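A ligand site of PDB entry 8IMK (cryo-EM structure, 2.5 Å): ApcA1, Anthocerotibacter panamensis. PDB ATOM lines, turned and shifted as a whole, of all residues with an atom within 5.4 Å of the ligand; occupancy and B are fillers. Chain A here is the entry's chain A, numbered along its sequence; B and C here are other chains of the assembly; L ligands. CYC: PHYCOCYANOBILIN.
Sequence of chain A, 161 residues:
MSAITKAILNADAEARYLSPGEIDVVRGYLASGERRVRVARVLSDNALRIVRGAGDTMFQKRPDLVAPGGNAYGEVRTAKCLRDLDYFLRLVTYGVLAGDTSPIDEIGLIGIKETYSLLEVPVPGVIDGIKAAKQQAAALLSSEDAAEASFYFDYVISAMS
OD1 of Asn 71 sits at hydrogen-bond distance from NC of the ligand, 2.5 Å away.
An oxygen (O1D) of the ligand lies within salt-bridge range of the guanidinium group of Arg 77 (2.7 Å).
OD2 of Asp 84 sits at hydrogen-bond distance from NA of the ligand (2.9 Å).
NZ of Lys 80 is in salt-bridge range of O1A of the ligand, at 2.9 Å.
NH1 of Arg 83 is in salt-bridge range of O2A of the ligand, 3.0 Å away.
The backbone carbonyl oxygen (O) of Asn 71 sits at hydrogen-bond distance from the guanidinium group (NE) of Arg 77 (2.5 Å).
The side-chain carboxylate of Asp 84 is in salt-bridge range of the guanidinium group of Arg 83.
OD2 of Asp 84 is in hydrogen-bond range of OH of Tyr 116 (2.8 Å).
OH of Tyr 74 of chain B lies within hydrogen-bond range of OD1 of Asp 13 of chain C, 2.8 Å away.
The backbone NH of Val 121 sits at hydrogen-bond distance from the backbone carbonyl oxygen of Tyr 116 (2.9 Å).
N of Ser 76 of chain B is in hydrogen-bond range of O of Ile 107 (3.3 Å).
The backbone carbonyl oxygen (O) of Leu 65 is in hydrogen-bond range of the backbone NH (N) of Ala 72 (3.0 Å).
The backbone carbonyl oxygen (O) of Ala 72 lies within hydrogen-bond range of the side-chain hydroxyl (OG1) of Thr 78, at 2.5 Å.
Merely in contact with the ligand: Met 58 (3.9 Å), Leu 65 (3.7 Å), Ala 72 (3.8 Å), Cys 81 (3.3 Å), Leu 85 (3.9 Å), Tyr 87 (3.4 Å), Phe 88 (3.6 Å), Ile 107 (3.6 Å), Ile 112 (3.7 Å), Thr 115 (3.8 Å), Tyr 116 (3.7 Å), Leu 119 (3.4 Å), Val 121 (3.5 Å), Pro 122 (3.6 Å), Gly 125 (3.6 Å), Val 126 (3.4 Å), Leu 67 of chain B (3.3 Å), Tyr 74 of chain B (3.4 Å), Thr 75 of chain B (3.6 Å) and Tyr 79 of chain B (3.4 Å).
Hydrophobic or aromatic side chains that line the ligand: Met 58, Leu 65, Ala 72, Leu 85, Tyr 87, Phe 88, Ile 112, Tyr 116, Leu 119, Val 121, Pro 122, Val 126, Leu 67 of chain B, Tyr 74 of chain B and Tyr 79 of chain B.
Within 4 Å of the ligand: Met 58, Leu 65, Asn 71, Ala 72, Arg 77, Lys 80, Cys 81, Arg 83, Asp 84, Leu 85, Tyr 87, Phe 88, Ile 107, Ile 112, Thr 115, Tyr 116, Leu 119, Val 121, Pro 122, Gly 125, Val 126, Leu 67 of chain B, Tyr 74 of chain B, Thr 75 of chain B and Tyr 79 of chain B.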
ATOM      1  N   MET A  58      -0.293  -2.684   3.946  1.00  0.00           N
ATOM      2  CA  MET A  58      -0.530  -1.462   3.186  1.00  0.00           C
ATOM      3  C   MET A  58      -1.992  -1.314   2.808  1.00  0.00           C
ATOM      4  O   MET A  58      -2.549  -0.209   2.892  1.00  0.00           O
ATOM      5  CB  MET A  58       0.364  -1.465   1.962  1.00  0.00           C
ATOM      6  CG  MET A  58       0.278  -0.247   1.084  1.00  0.00           C
ATOM      7  SD  MET A  58       1.426  -0.462  -0.270  1.00  0.00           S
ATOM      8  CE  MET A  58       0.575  -1.720  -1.176  1.00  0.00           C
ATOM      9  N   LEU A  65      -6.750   2.337  -1.899  1.00  0.00           N
ATOM     10  CA  LEU A  65      -5.994   1.943  -3.087  1.00  0.00           C
ATOM     11  C   LEU A  65      -6.642   0.763  -3.796  1.00  0.00           C
ATOM     12  O   LEU A  65      -6.688   0.712  -5.033  1.00  0.00           O
ATOM     13  CB  LEU A  65      -4.558   1.610  -2.699  1.00  0.00           C
ATOM     14  CG  LEU A  65      -3.750   2.717  -2.023  1.00  0.00           C
ATOM     15  CD1 LEU A  65      -2.367   2.221  -1.705  1.00  0.00           C
ATOM     16  CD2 LEU A  65      -3.700   3.938  -2.907  1.00  0.00           C
ATOM     17  N   ASN A  71      -5.984   3.403  -7.143  1.00  0.00           N
ATOM     18  CA  ASN A  71      -4.965   3.175  -8.158  1.00  0.00           C
ATOM     19  C   ASN A  71      -4.710   1.692  -8.372  1.00  0.00           C
ATOM     20  O   ASN A  71      -4.481   1.256  -9.503  1.00  0.00           O
ATOM     21  CB  ASN A  71      -3.669   3.901  -7.771  1.00  0.00           C
ATOM     22  CG  ASN A  71      -2.489   3.481  -8.613  1.00  0.00           C
ATOM     23  OD1 ASN A  71      -1.617   2.738  -8.168  1.00  0.00           O
ATOM     24  ND2 ASN A  71      -2.448   3.951  -9.857  1.00  0.00           N
ATOM     25  N   ALA A  72      -4.752   0.908  -7.308  1.00  0.00           N
ATOM     26  CA  ALA A  72      -4.515  -0.527  -7.392  1.00  0.00           C
ATOM     27  C   ALA A  72      -5.800  -1.330  -7.449  1.00  0.00           C
ATOM     28  O   ALA A  72      -5.789  -2.519  -7.112  1.00  0.00           O
ATOM     29  CB  ALA A  72      -3.656  -0.995  -6.222  1.00  0.00           C
ATOM     30  N   ARG A  77      -4.234  -4.790 -11.398  1.00  0.00           N
ATOM     31  CA  ARG A  77      -3.533  -3.625 -10.879  1.00  0.00           C
ATOM     32  C   ARG A  77      -2.985  -3.911  -9.484  1.00  0.00           C
ATOM     33  O   ARG A  77      -1.888  -3.459  -9.128  1.00  0.00           O
ATOM     34  CB  ARG A  77      -4.478  -2.424 -10.883  1.00  0.00           C
ATOM     35  CG  ARG A  77      -4.868  -1.978 -12.287  1.00  0.00           C
ATOM     36  CD  ARG A  77      -5.866  -0.836 -12.288  1.00  0.00           C
ATOM     37  NE  ARG A  77      -5.361   0.415 -11.731  1.00  0.00           N
ATOM     38  CZ  ARG A  77      -4.724   1.340 -12.455  1.00  0.00           C
ATOM     39  NH1 ARG A  77      -4.295   2.454 -11.869  1.00  0.00           N
ATOM     40  NH2 ARG A  77      -4.574   1.174 -13.759  1.00  0.00           N
ATOM     41  N   THR A  78      -3.723  -4.686  -8.683  1.00  0.00           N
ATOM     42  CA  THR A  78      -3.206  -5.106  -7.377  1.00  0.00           C
ATOM     43  C   THR A  78      -2.005  -6.021  -7.538  1.00  0.00           C
ATOM     44  O   THR A  78      -1.043  -5.935  -6.758  1.00  0.00           O
ATOM     45  CB  THR A  78      -4.315  -5.790  -6.580  1.00  0.00           C
ATOM     46  OG1 THR A  78      -5.483  -4.972  -6.561  1.00  0.00           O
ATOM     47  CG2 THR A  78      -3.859  -6.020  -5.155  1.00  0.00           C
ATOM     48  N   LYS A  80       0.094  -5.844  -9.993  1.00  0.00           N
ATOM     49  CA  LYS A  80       1.182  -4.944 -10.351  1.00  0.00           C
ATOM     50  C   LYS A  80       1.739  -4.212  -9.138  1.00  0.00           C
ATOM     51  O   LYS A  80       2.951  -4.001  -9.026  1.00  0.00           O
ATOM     52  CB  LYS A  80       0.712  -3.934 -11.397  1.00  0.00           C
ATOM     53  CG  LYS A  80       0.403  -4.524 -12.736  1.00  0.00           C
ATOM     54  CD  LYS A  80       0.704  -3.549 -13.836  1.00  0.00           C
ATOM     55  CE  LYS A  80      -0.055  -3.898 -15.090  1.00  0.00           C
ATOM     56  NZ  LYS A  80       0.069  -2.821 -16.108  1.00  0.00           N
ATOM     57  N   CYS A  81       0.861  -3.820  -8.217  1.00  0.00           N
ATOM     58  CA  CYS A  81       1.307  -3.211  -6.969  1.00  0.00           C
ATOM     59  C   CYS A  81       2.180  -4.154  -6.157  1.00  0.00           C
ATOM     60  O   CYS A  81       3.258  -3.762  -5.664  1.00  0.00           O
ATOM     61  CB  CYS A  81       0.071  -2.781  -6.178  1.00  0.00           C
ATOM     62  SG  CYS A  81       0.330  -2.247  -4.513  1.00  0.00           S
ATOM     63  N   ARG A  83       3.821  -6.634  -7.337  1.00  0.00           N
ATOM     64  CA  ARG A  83       5.033  -6.831  -8.117  1.00  0.00           C
ATOM     65  C   ARG A  83       6.013  -5.686  -7.901  1.00  0.00           C
ATOM     66  O   ARG A  83       7.227  -5.897  -7.894  1.00  0.00           O
ATOM     67  CB  ARG A  83       4.664  -6.968  -9.589  1.00  0.00           C
ATOM     68  CG  ARG A  83       5.825  -6.865 -10.552  1.00  0.00           C
ATOM     69  CD  ARG A  83       5.392  -6.207 -11.827  1.00  0.00           C
ATOM     70  NE  ARG A  83       5.310  -4.754 -11.705  1.00  0.00           N
ATOM     71  CZ  ARG A  83       4.770  -3.958 -12.609  1.00  0.00           C
ATOM     72  NH1 ARG A  83       4.256  -4.467 -13.720  1.00  0.00           N
ATOM     73  NH2 ARG A  83       4.750  -2.658 -12.416  1.00  0.00           N
ATOM     74  N   ASP A  84       5.507  -4.462  -7.714  1.00  0.00           N
ATOM     75  CA  ASP A  84       6.397  -3.353  -7.418  1.00  0.00           C
ATOM     76  C   ASP A  84       7.018  -3.506  -6.040  1.00  0.00           C
ATOM     77  O   ASP A  84       8.209  -3.205  -5.838  1.00  0.00           O
ATOM     78  CB  ASP A  84       5.652  -2.023  -7.508  1.00  0.00           C
ATOM     79  CG  ASP A  84       5.371  -1.625  -8.930  1.00  0.00           C
ATOM     80  OD1 ASP A  84       5.551  -2.469  -9.829  1.00  0.00           O
ATOM     81  OD2 ASP A  84       4.972  -0.474  -9.149  1.00  0.00           O
ATOM     82  N   LEU A  85       6.241  -3.980  -5.068  1.00  0.00           N
ATOM     83  CA  LEU A  85       6.824  -4.252  -3.754  1.00  0.00           C
ATOM     84  C   LEU A  85       7.887  -5.337  -3.845  1.00  0.00           C
ATOM     85  O   LEU A  85       8.945  -5.238  -3.202  1.00  0.00           O
ATOM     86  CB  LEU A  85       5.730  -4.652  -2.769  1.00  0.00           C
ATOM     87  CG  LEU A  85       4.816  -3.533  -2.292  1.00  0.00           C
ATOM     88  CD1 LEU A  85       3.816  -4.037  -1.262  1.00  0.00           C
ATOM     89  CD2 LEU A  85       5.630  -2.391  -1.716  1.00  0.00           C
ATOM     90  N   TYR A  87       9.697  -5.915  -6.491  1.00  0.00           N
ATOM     91  CA  TYR A  87      10.812  -5.255  -7.137  1.00  0.00           C
ATOM     92  C   TYR A  87      11.680  -4.543  -6.117  1.00  0.00           C
ATOM     93  O   TYR A  87      12.911  -4.640  -6.150  1.00  0.00           O
ATOM     94  CB  TYR A  87      10.311  -4.254  -8.176  1.00  0.00           C
ATOM     95  CG  TYR A  87       9.866  -4.852  -9.473  1.00  0.00           C
ATOM     96  CD1 TYR A  87      10.065  -6.191  -9.759  1.00  0.00           C
ATOM     97  CD2 TYR A  87       9.220  -4.067 -10.419  1.00  0.00           C
ATOM     98  CE1 TYR A  87       9.652  -6.731 -10.944  1.00  0.00           C
ATOM     99  CE2 TYR A  87       8.809  -4.603 -11.618  1.00  0.00           C
ATOM    100  CZ  TYR A  87       9.034  -5.931 -11.874  1.00  0.00           C
ATOM    101  OH  TYR A  87       8.621  -6.470 -13.059  1.00  0.00           O
ATOM    102  N   PHE A  88      11.047  -3.819  -5.201  1.00  0.00           N
ATOM    103  CA  PHE A  88      11.819  -3.010  -4.259  1.00  0.00           C
ATOM    104  C   PHE A  88      12.502  -3.887  -3.214  1.00  0.00           C
ATOM    105  O   PHE A  88      13.610  -3.573  -2.783  1.00  0.00           O
ATOM    106  CB  PHE A  88      10.925  -1.953  -3.633  1.00  0.00           C
ATOM    107  CG  PHE A  88      10.620  -0.827  -4.559  1.00  0.00           C
ATOM    108  CD1 PHE A  88      11.642  -0.164  -5.212  1.00  0.00           C
ATOM    109  CD2 PHE A  88       9.323  -0.455  -4.823  1.00  0.00           C
ATOM    110  CE1 PHE A  88      11.378   0.859  -6.086  1.00  0.00           C
ATOM    111  CE2 PHE A  88       9.057   0.555  -5.694  1.00  0.00           C
ATOM    112  CZ  PHE A  88      10.089   1.221  -6.329  1.00  0.00           C
ATOM    113  N   ARG A  90      13.637  -6.920  -3.885  1.00  0.00           N
ATOM    114  CA  ARG A  90      14.772  -7.501  -4.594  1.00  0.00           C
ATOM    115  C   ARG A  90      15.893  -6.472  -4.760  1.00  0.00           C
ATOM    116  O   ARG A  90      17.074  -6.810  -4.691  1.00  0.00           O
ATOM    117  CB  ARG A  90      14.322  -8.045  -5.943  1.00  0.00           C
ATOM    118  CG  ARG A  90      15.419  -8.807  -6.637  1.00  0.00           C
ATOM    119  CD  ARG A  90      14.900  -9.581  -7.818  1.00  0.00           C
ATOM    120  NE  ARG A  90      13.949  -8.813  -8.604  1.00  0.00           N
ATOM    121  CZ  ARG A  90      14.261  -8.140  -9.707  1.00  0.00           C
ATOM    122  NH1 ARG A  90      15.499  -8.154 -10.161  1.00  0.00           N
ATOM    123  NH2 ARG A  90      13.321  -7.473 -10.356  1.00  0.00           N
ATOM    124  N   LEU A  91      15.527  -5.206  -4.970  1.00  0.00           N
ATOM    125  CA  LEU A  91      16.526  -4.162  -5.048  1.00  0.00           C
ATOM    126  C   LEU A  91      17.206  -3.950  -3.704  1.00  0.00           C
ATOM    127  O   LEU A  91      18.407  -3.651  -3.657  1.00  0.00           O
ATOM    128  CB  LEU A  91      15.903  -2.862  -5.536  1.00  0.00           C
ATOM    129  CG  LEU A  91      15.498  -2.891  -7.005  1.00  0.00           C
ATOM    130  CD1 LEU A  91      15.204  -1.497  -7.472  1.00  0.00           C
ATOM    131  CD2 LEU A  91      16.581  -3.517  -7.840  1.00  0.00           C
ATOM    132  N   ILE A 107      18.571   0.436 -11.275  1.00  0.00           N
ATOM    133  CA  ILE A 107      17.482  -0.422 -11.732  1.00  0.00           C
ATOM    134  C   ILE A 107      16.131   0.204 -11.418  1.00  0.00           C
ATOM    135  O   ILE A 107      15.223   0.222 -12.256  1.00  0.00           O
ATOM    136  CB  ILE A 107      17.598  -1.833 -11.129  1.00  0.00           C
ATOM    137  CG1 ILE A 107      18.904  -2.499 -11.573  1.00  0.00           C
ATOM    138  CG2 ILE A 107      16.424  -2.688 -11.562  1.00  0.00           C
ATOM    139  CD1 ILE A 107      19.381  -3.559 -10.615  1.00  0.00           C
ATOM    140  N   GLY A 108      15.975   0.756 -10.219  1.00  0.00           N
ATOM    141  CA  GLY A 108      14.629   1.075  -9.777  1.00  0.00           C
ATOM    142  C   GLY A 108      14.296   2.485  -9.358  1.00  0.00           C
ATOM    143  O   GLY A 108      13.129   2.863  -9.406  1.00  0.00           O
ATOM    144  N   ILE A 112      11.823   6.818 -11.008  1.00  0.00           N
ATOM    145  CA  ILE A 112      10.641   6.238 -10.373  1.00  0.00           C
ATOM    146  C   ILE A 112       9.673   7.322  -9.953  1.00  0.00           C
ATOM    147  O   ILE A 112       8.451   7.125  -9.981  1.00  0.00           O
ATOM    148  CB  ILE A 112      11.039   5.326  -9.199  1.00  0.00           C
ATOM    149  CG1 ILE A 112       9.867   4.409  -8.838  1.00  0.00           C
ATOM    150  CG2 ILE A 112      11.425   6.128  -7.972  1.00  0.00           C
ATOM    151  CD1 ILE A 112       9.383   3.576  -9.970  1.00  0.00           C
ATOM    152  N   THR A 115       7.786   8.644 -12.828  1.00  0.00           N
ATOM    153  CA  THR A 115       6.991   7.521 -13.313  1.00  0.00           C
ATOM    154  C   THR A 115       5.697   7.390 -12.515  1.00  0.00           C
ATOM    155  O   THR A 115       4.602   7.372 -13.082  1.00  0.00           O
ATOM    156  CB  THR A 115       7.790   6.224 -13.212  1.00  0.00           C
ATOM    157  OG1 THR A 115       8.980   6.336 -13.996  1.00  0.00           O
ATOM    158  CG2 THR A 115       6.973   5.052 -13.700  1.00  0.00           C
ATOM    159  N   TYR A 116       5.826   7.333 -11.191  1.00  0.00           N
ATOM    160  CA  TYR A 116       4.639   7.212 -10.350  1.00  0.00           C
ATOM    161  C   TYR A 116       3.764   8.462 -10.447  1.00  0.00           C
ATOM    162  O   TYR A 116       2.541   8.354 -10.443  1.00  0.00           O
ATOM    163  CB  TYR A 116       5.047   6.950  -8.905  1.00  0.00           C
ATOM    164  CG  TYR A 116       5.388   5.502  -8.639  1.00  0.00           C
ATOM    165  CD1 TYR A 116       4.951   4.490  -9.480  1.00  0.00           C
ATOM    166  CD2 TYR A 116       6.137   5.144  -7.530  1.00  0.00           C
ATOM    167  CE1 TYR A 116       5.248   3.185  -9.226  1.00  0.00           C
ATOM    168  CE2 TYR A 116       6.439   3.841  -7.267  1.00  0.00           C
ATOM    169  CZ  TYR A 116       5.989   2.858  -8.117  1.00  0.00           C
ATOM    170  OH  TYR A 116       6.308   1.552  -7.852  1.00  0.00           O
ATOM    171  N   LEU A 119       1.777   8.075 -13.579  1.00  0.00           N
ATOM    172  CA  LEU A 119       0.791   7.022 -13.472  1.00  0.00           C
ATOM    173  C   LEU A 119      -0.197   7.235 -12.345  1.00  0.00           C
ATOM    174  O   LEU A 119      -1.034   6.357 -12.096  1.00  0.00           O
ATOM    175  CB  LEU A 119       1.483   5.674 -13.269  1.00  0.00           C
ATOM    176  CG  LEU A 119       2.280   5.173 -14.451  1.00  0.00           C
ATOM    177  CD1 LEU A 119       3.439   4.387 -13.904  1.00  0.00           C
ATOM    178  CD2 LEU A 119       1.421   4.314 -15.348  1.00  0.00           C
ATOM    179  N   VAL A 121       0.287   7.083  -9.238  1.00  0.00           N
ATOM    180  CA  VAL A 121       0.523   6.145  -8.143  1.00  0.00           C
ATOM    181  C   VAL A 121       0.857   6.932  -6.885  1.00  0.00           C
ATOM    182  O   VAL A 121       1.811   7.733  -6.898  1.00  0.00           O
ATOM    183  CB  VAL A 121       1.647   5.181  -8.495  1.00  0.00           C
ATOM    184  CG1 VAL A 121       2.149   4.487  -7.241  1.00  0.00           C
ATOM    185  CG2 VAL A 121       1.161   4.158  -9.504  1.00  0.00           C
ATOM    186  N   PRO A 122       0.110   6.753  -5.793  1.00  0.00           N
ATOM    187  CA  PRO A 122       0.380   7.506  -4.563  1.00  0.00           C
ATOM    188  C   PRO A 122       1.695   7.064  -3.928  1.00  0.00           C
ATOM    189  O   PRO A 122       1.850   5.900  -3.560  1.00  0.00           O
ATOM    190  CB  PRO A 122      -0.820   7.165  -3.668  1.00  0.00           C
ATOM    191  CG  PRO A 122      -1.837   6.579  -4.579  1.00  0.00           C
ATOM    192  CD  PRO A 122      -1.091   5.922  -5.673  1.00  0.00           C
ATOM    193  N   GLY A 125       1.439   5.697  -0.363  1.00  0.00           N
ATOM    194  CA  GLY A 125       1.090   4.282  -0.344  1.00  0.00           C
ATOM    195  C   GLY A 125       2.295   3.391  -0.558  1.00  0.00           C
ATOM    196  O   GLY A 125       2.477   2.404   0.172  1.00  0.00           O
ATOM    197  N   VAL A 126       3.135   3.725  -1.529  1.00  0.00           N
ATOM    198  CA  VAL A 126       4.336   2.922  -1.778  1.00  0.00           C
ATOM    199  C   VAL A 126       5.250   2.957  -0.558  1.00  0.00           C
ATOM    200  O   VAL A 126       5.828   1.936  -0.183  1.00  0.00           O
ATOM    201  CB  VAL A 126       5.078   3.424  -3.023  1.00  0.00           C
ATOM    202  CG1 VAL A 126       6.140   2.419  -3.427  1.00  0.00           C
ATOM    203  CG2 VAL A 126       4.124   3.684  -4.164  1.00  0.00           C
ATOM    204  N   PHE B  60       1.656  -0.799 -23.824  1.00  0.00           N
ATOM    205  CA  PHE B  60       2.188  -1.834 -22.947  1.00  0.00           C
ATOM    206  C   PHE B  60       1.158  -2.932 -22.681  1.00  0.00           C
ATOM    207  O   PHE B  60       1.506  -4.017 -22.213  1.00  0.00           O
ATOM    208  CB  PHE B  60       2.691  -1.196 -21.666  1.00  0.00           C
ATOM    209  CG  PHE B  60       3.880  -0.329 -21.889  1.00  0.00           C
ATOM    210  CD1 PHE B  60       4.935  -0.781 -22.657  1.00  0.00           C
ATOM    211  CD2 PHE B  60       3.927   0.956 -21.385  1.00  0.00           C
ATOM    212  CE1 PHE B  60       6.029   0.003 -22.883  1.00  0.00           C
ATOM    213  CE2 PHE B  60       5.023   1.743 -21.624  1.00  0.00           C
ATOM    214  CZ  PHE B  60       6.067   1.268 -22.370  1.00  0.00           C
ATOM    215  N   LEU B  67       7.902  -4.460 -20.878  1.00  0.00           N
ATOM    216  CA  LEU B  67       8.066  -4.155 -19.459  1.00  0.00           C
ATOM    217  C   LEU B  67       8.772  -5.283 -18.721  1.00  0.00           C
ATOM    218  O   LEU B  67       9.370  -5.046 -17.659  1.00  0.00           O
ATOM    219  CB  LEU B  67       6.698  -3.881 -18.847  1.00  0.00           C
ATOM    220  CG  LEU B  67       6.002  -2.638 -19.401  1.00  0.00           C
ATOM    221  CD1 LEU B  67       4.718  -2.405 -18.668  1.00  0.00           C
ATOM    222  CD2 LEU B  67       6.901  -1.415 -19.302  1.00  0.00           C
ATOM    223  N   ALA B  73      11.929  -1.705 -22.061  1.00  0.00           N
ATOM    224  CA  ALA B  73      11.281  -0.758 -21.173  1.00  0.00           C
ATOM    225  C   ALA B  73      11.324  -1.203 -19.715  1.00  0.00           C
ATOM    226  O   ALA B  73      10.650  -0.596 -18.884  1.00  0.00           O
ATOM    227  CB  ALA B  73       9.835  -0.530 -21.608  1.00  0.00           C
ATOM    228  N   TYR B  74      12.109  -2.218 -19.385  1.00  0.00           N
ATOM    229  CA  TYR B  74      12.207  -2.675 -18.003  1.00  0.00           C
ATOM    230  C   TYR B  74      13.327  -1.955 -17.274  1.00  0.00           C
ATOM    231  O   TYR B  74      14.508  -2.300 -17.424  1.00  0.00           O
ATOM    232  CB  TYR B  74      12.457  -4.178 -17.933  1.00  0.00           C
ATOM    233  CG  TYR B  74      12.860  -4.646 -16.555  1.00  0.00           C
ATOM    234  CD1 TYR B  74      11.912  -4.791 -15.554  1.00  0.00           C
ATOM    235  CD2 TYR B  74      14.184  -4.926 -16.252  1.00  0.00           C
ATOM    236  CE1 TYR B  74      12.279  -5.211 -14.303  1.00  0.00           C
ATOM    237  CE2 TYR B  74      14.547  -5.324 -15.003  1.00  0.00           C
ATOM    238  CZ  TYR B  74      13.602  -5.474 -14.025  1.00  0.00           C
ATOM    239  OH  TYR B  74      13.970  -5.881 -12.777  1.00  0.00           O
ATOM    240  N   THR B  75      12.962  -0.876 -16.599  1.00  0.00           N
ATOM    241  CA  THR B  75      13.528  -0.283 -15.381  1.00  0.00           C
ATOM    242  C   THR B  75      12.709   0.968 -15.163  1.00  0.00           C
ATOM    243  O   THR B  75      11.916   1.337 -16.030  1.00  0.00           O
ATOM    244  CB  THR B  75      15.031   0.033 -15.435  1.00  0.00           C
ATOM    245  OG1 THR B  75      15.349   0.730 -16.650  1.00  0.00           O
ATOM    246  CG2 THR B  75      15.919  -1.186 -15.200  1.00  0.00           C
ATOM    247  N   SER B  76      12.852   1.621 -14.020  1.00  0.00           N
ATOM    248  CA  SER B  76      12.173   2.898 -13.861  1.00  0.00           C
ATOM    249  C   SER B  76      12.727   3.927 -14.844  1.00  0.00           C
ATOM    250  O   SER B  76      11.971   4.719 -15.419  1.00  0.00           O
ATOM    251  CB  SER B  76      12.290   3.398 -12.424  1.00  0.00           C
ATOM    252  OG  SER B  76      13.537   4.013 -12.188  1.00  0.00           O
ATOM    253  N   TYR B  79      11.680   2.953 -18.599  1.00  0.00           N
ATOM    254  CA  TYR B  79      10.273   3.289 -18.773  1.00  0.00           C
ATOM    255  C   TYR B  79      10.072   4.799 -18.848  1.00  0.00           C
ATOM    256  O   TYR B  79       9.311   5.303 -19.686  1.00  0.00           O
ATOM    257  CB  TYR B  79       9.455   2.698 -17.633  1.00  0.00           C
ATOM    258  CG  TYR B  79       7.995   3.042 -17.709  1.00  0.00           C
ATOM    259  CD1 TYR B  79       7.114   2.240 -18.407  1.00  0.00           C
ATOM    260  CD2 TYR B  79       7.498   4.182 -17.098  1.00  0.00           C
ATOM    261  CE1 TYR B  79       5.789   2.562 -18.497  1.00  0.00           C
ATOM    262  CE2 TYR B  79       6.170   4.501 -17.174  1.00  0.00           C
ATOM    263  CZ  TYR B  79       5.317   3.680 -17.873  1.00  0.00           C
ATOM    264  OH  TYR B  79       3.985   3.987 -17.968  1.00  0.00           O
ATOM    265  N   ASP C  13      19.034  -9.662 -12.402  1.00  0.00           N
ATOM    266  CA  ASP C  13      18.081  -8.627 -12.768  1.00  0.00           C
ATOM    267  C   ASP C  13      17.615  -8.808 -14.202  1.00  0.00           C
ATOM    268  O   ASP C  13      16.511  -8.403 -14.566  1.00  0.00           O
ATOM    269  CB  ASP C  13      18.706  -7.248 -12.565  1.00  0.00           C
ATOM    270  CG  ASP C  13      17.800  -6.123 -12.995  1.00  0.00           C
ATOM    271  OD1 ASP C  13      16.704  -5.982 -12.420  1.00  0.00           O
ATOM    272  OD2 ASP C  13      18.177  -5.382 -13.926  1.00  0.00           O
HETATM  273  CHA CYC L   1       2.512   0.599 -12.936  1.00  0.00           C
HETATM  274  NA  CYC L   1       4.862   0.378 -11.873  1.00  0.00           N
HETATM  275  C1A CYC L   1       4.080   0.661 -12.882  1.00  0.00           C
HETATM  276  C2A CYC L   1       4.862   1.037 -13.955  1.00  0.00           C
HETATM  277  C3A CYC L   1       6.177   0.966 -13.519  1.00  0.00           C
HETATM  278  C4A CYC L   1       6.133   0.538 -12.189  1.00  0.00           C
HETATM  279  CMA CYC L   1       7.358   1.325 -14.442  1.00  0.00           C
HETATM  280  CAA CYC L   1       4.395   1.471 -15.361  1.00  0.00           C
HETATM  281  CBA CYC L   1       4.360   0.264 -16.371  1.00  0.00           C
HETATM  282  CGA CYC L   1       3.625  -1.009 -15.779  1.00  0.00           C
HETATM  283  O1A CYC L   1       2.351  -1.022 -15.681  1.00  0.00           O
HETATM  284  O2A CYC L   1       4.305  -2.033 -15.425  1.00  0.00           O
HETATM  285  CHB CYC L   1       7.352   0.271 -11.148  1.00  0.00           C
HETATM  286  NB  CYC L   1       8.732  -0.918 -12.901  1.00  0.00           N
HETATM  287  C1B CYC L   1       8.594  -0.387 -11.720  1.00  0.00           C
HETATM  288  C2B CYC L   1       9.772  -0.526 -11.058  1.00  0.00           C
HETATM  289  C3B CYC L   1      10.645  -1.182 -11.922  1.00  0.00           C
HETATM  290  C4B CYC L   1       9.943  -1.396 -13.069  1.00  0.00           C
HETATM  291  CMB CYC L   1      10.082  -0.057  -9.642  1.00  0.00           C
HETATM  292  CAB CYC L   1      12.149  -1.581 -11.654  1.00  0.00           C
HETATM  293  CBB CYC L   1      12.345  -3.053 -11.420  1.00  0.00           C
HETATM  294  OB  CYC L   1      10.429  -2.042 -14.263  1.00  0.00           O
HETATM  295  NC  CYC L   1      -0.239   0.994  -6.930  1.00  0.00           N
HETATM  296  C1C CYC L   1      -0.643   1.227  -5.484  1.00  0.00           C
HETATM  297  C2C CYC L   1       0.735   1.198  -4.615  1.00  0.00           C
HETATM  298  C3C CYC L   1       1.698   1.213  -5.443  1.00  0.00           C
HETATM  299  C4C CYC L   1       1.073   1.173  -7.018  1.00  0.00           C
HETATM  300  CMC CYC L   1       0.765   2.500  -3.676  1.00  0.00           C
HETATM  301  CAC CYC L   1       2.680  -0.019  -5.210  1.00  0.00           C
HETATM  302  CBC CYC L   1       3.126  -0.215  -3.740  1.00  0.00           C
HETATM  303  OC  CYC L   1      -1.205   2.333  -5.363  1.00  0.00           O
HETATM  304  CHD CYC L   1       1.735   0.076  -7.821  1.00  0.00           C
HETATM  305  ND  CYC L   1       2.357   0.375 -10.307  1.00  0.00           N
HETATM  306  C1D CYC L   1       1.420   0.158  -9.392  1.00  0.00           C
HETATM  307  C2D CYC L   1       0.183  -0.003 -10.053  1.00  0.00           C
HETATM  308  C3D CYC L   1       0.447   0.149 -11.404  1.00  0.00           C
HETATM  309  C4D CYC L   1       1.809   0.375 -11.515  1.00  0.00           C
HETATM  310  CMD CYC L   1      -1.240  -0.291  -9.493  1.00  0.00           C
HETATM  311  CAD CYC L   1      -0.557   0.070 -12.555  1.00  0.00           C
HETATM  312  CBD CYC L   1      -1.111   1.466 -12.877  1.00  0.00           C
HETATM  313  CGD CYC L   1      -1.611   1.574 -14.315  1.00  0.00           C
HETATM  314  O1D CYC L   1      -2.423   2.489 -14.648  1.00  0.00           O
HETATM  315  O2D CYC L   1      -1.221   0.745 -15.160  1.00  0.00           O
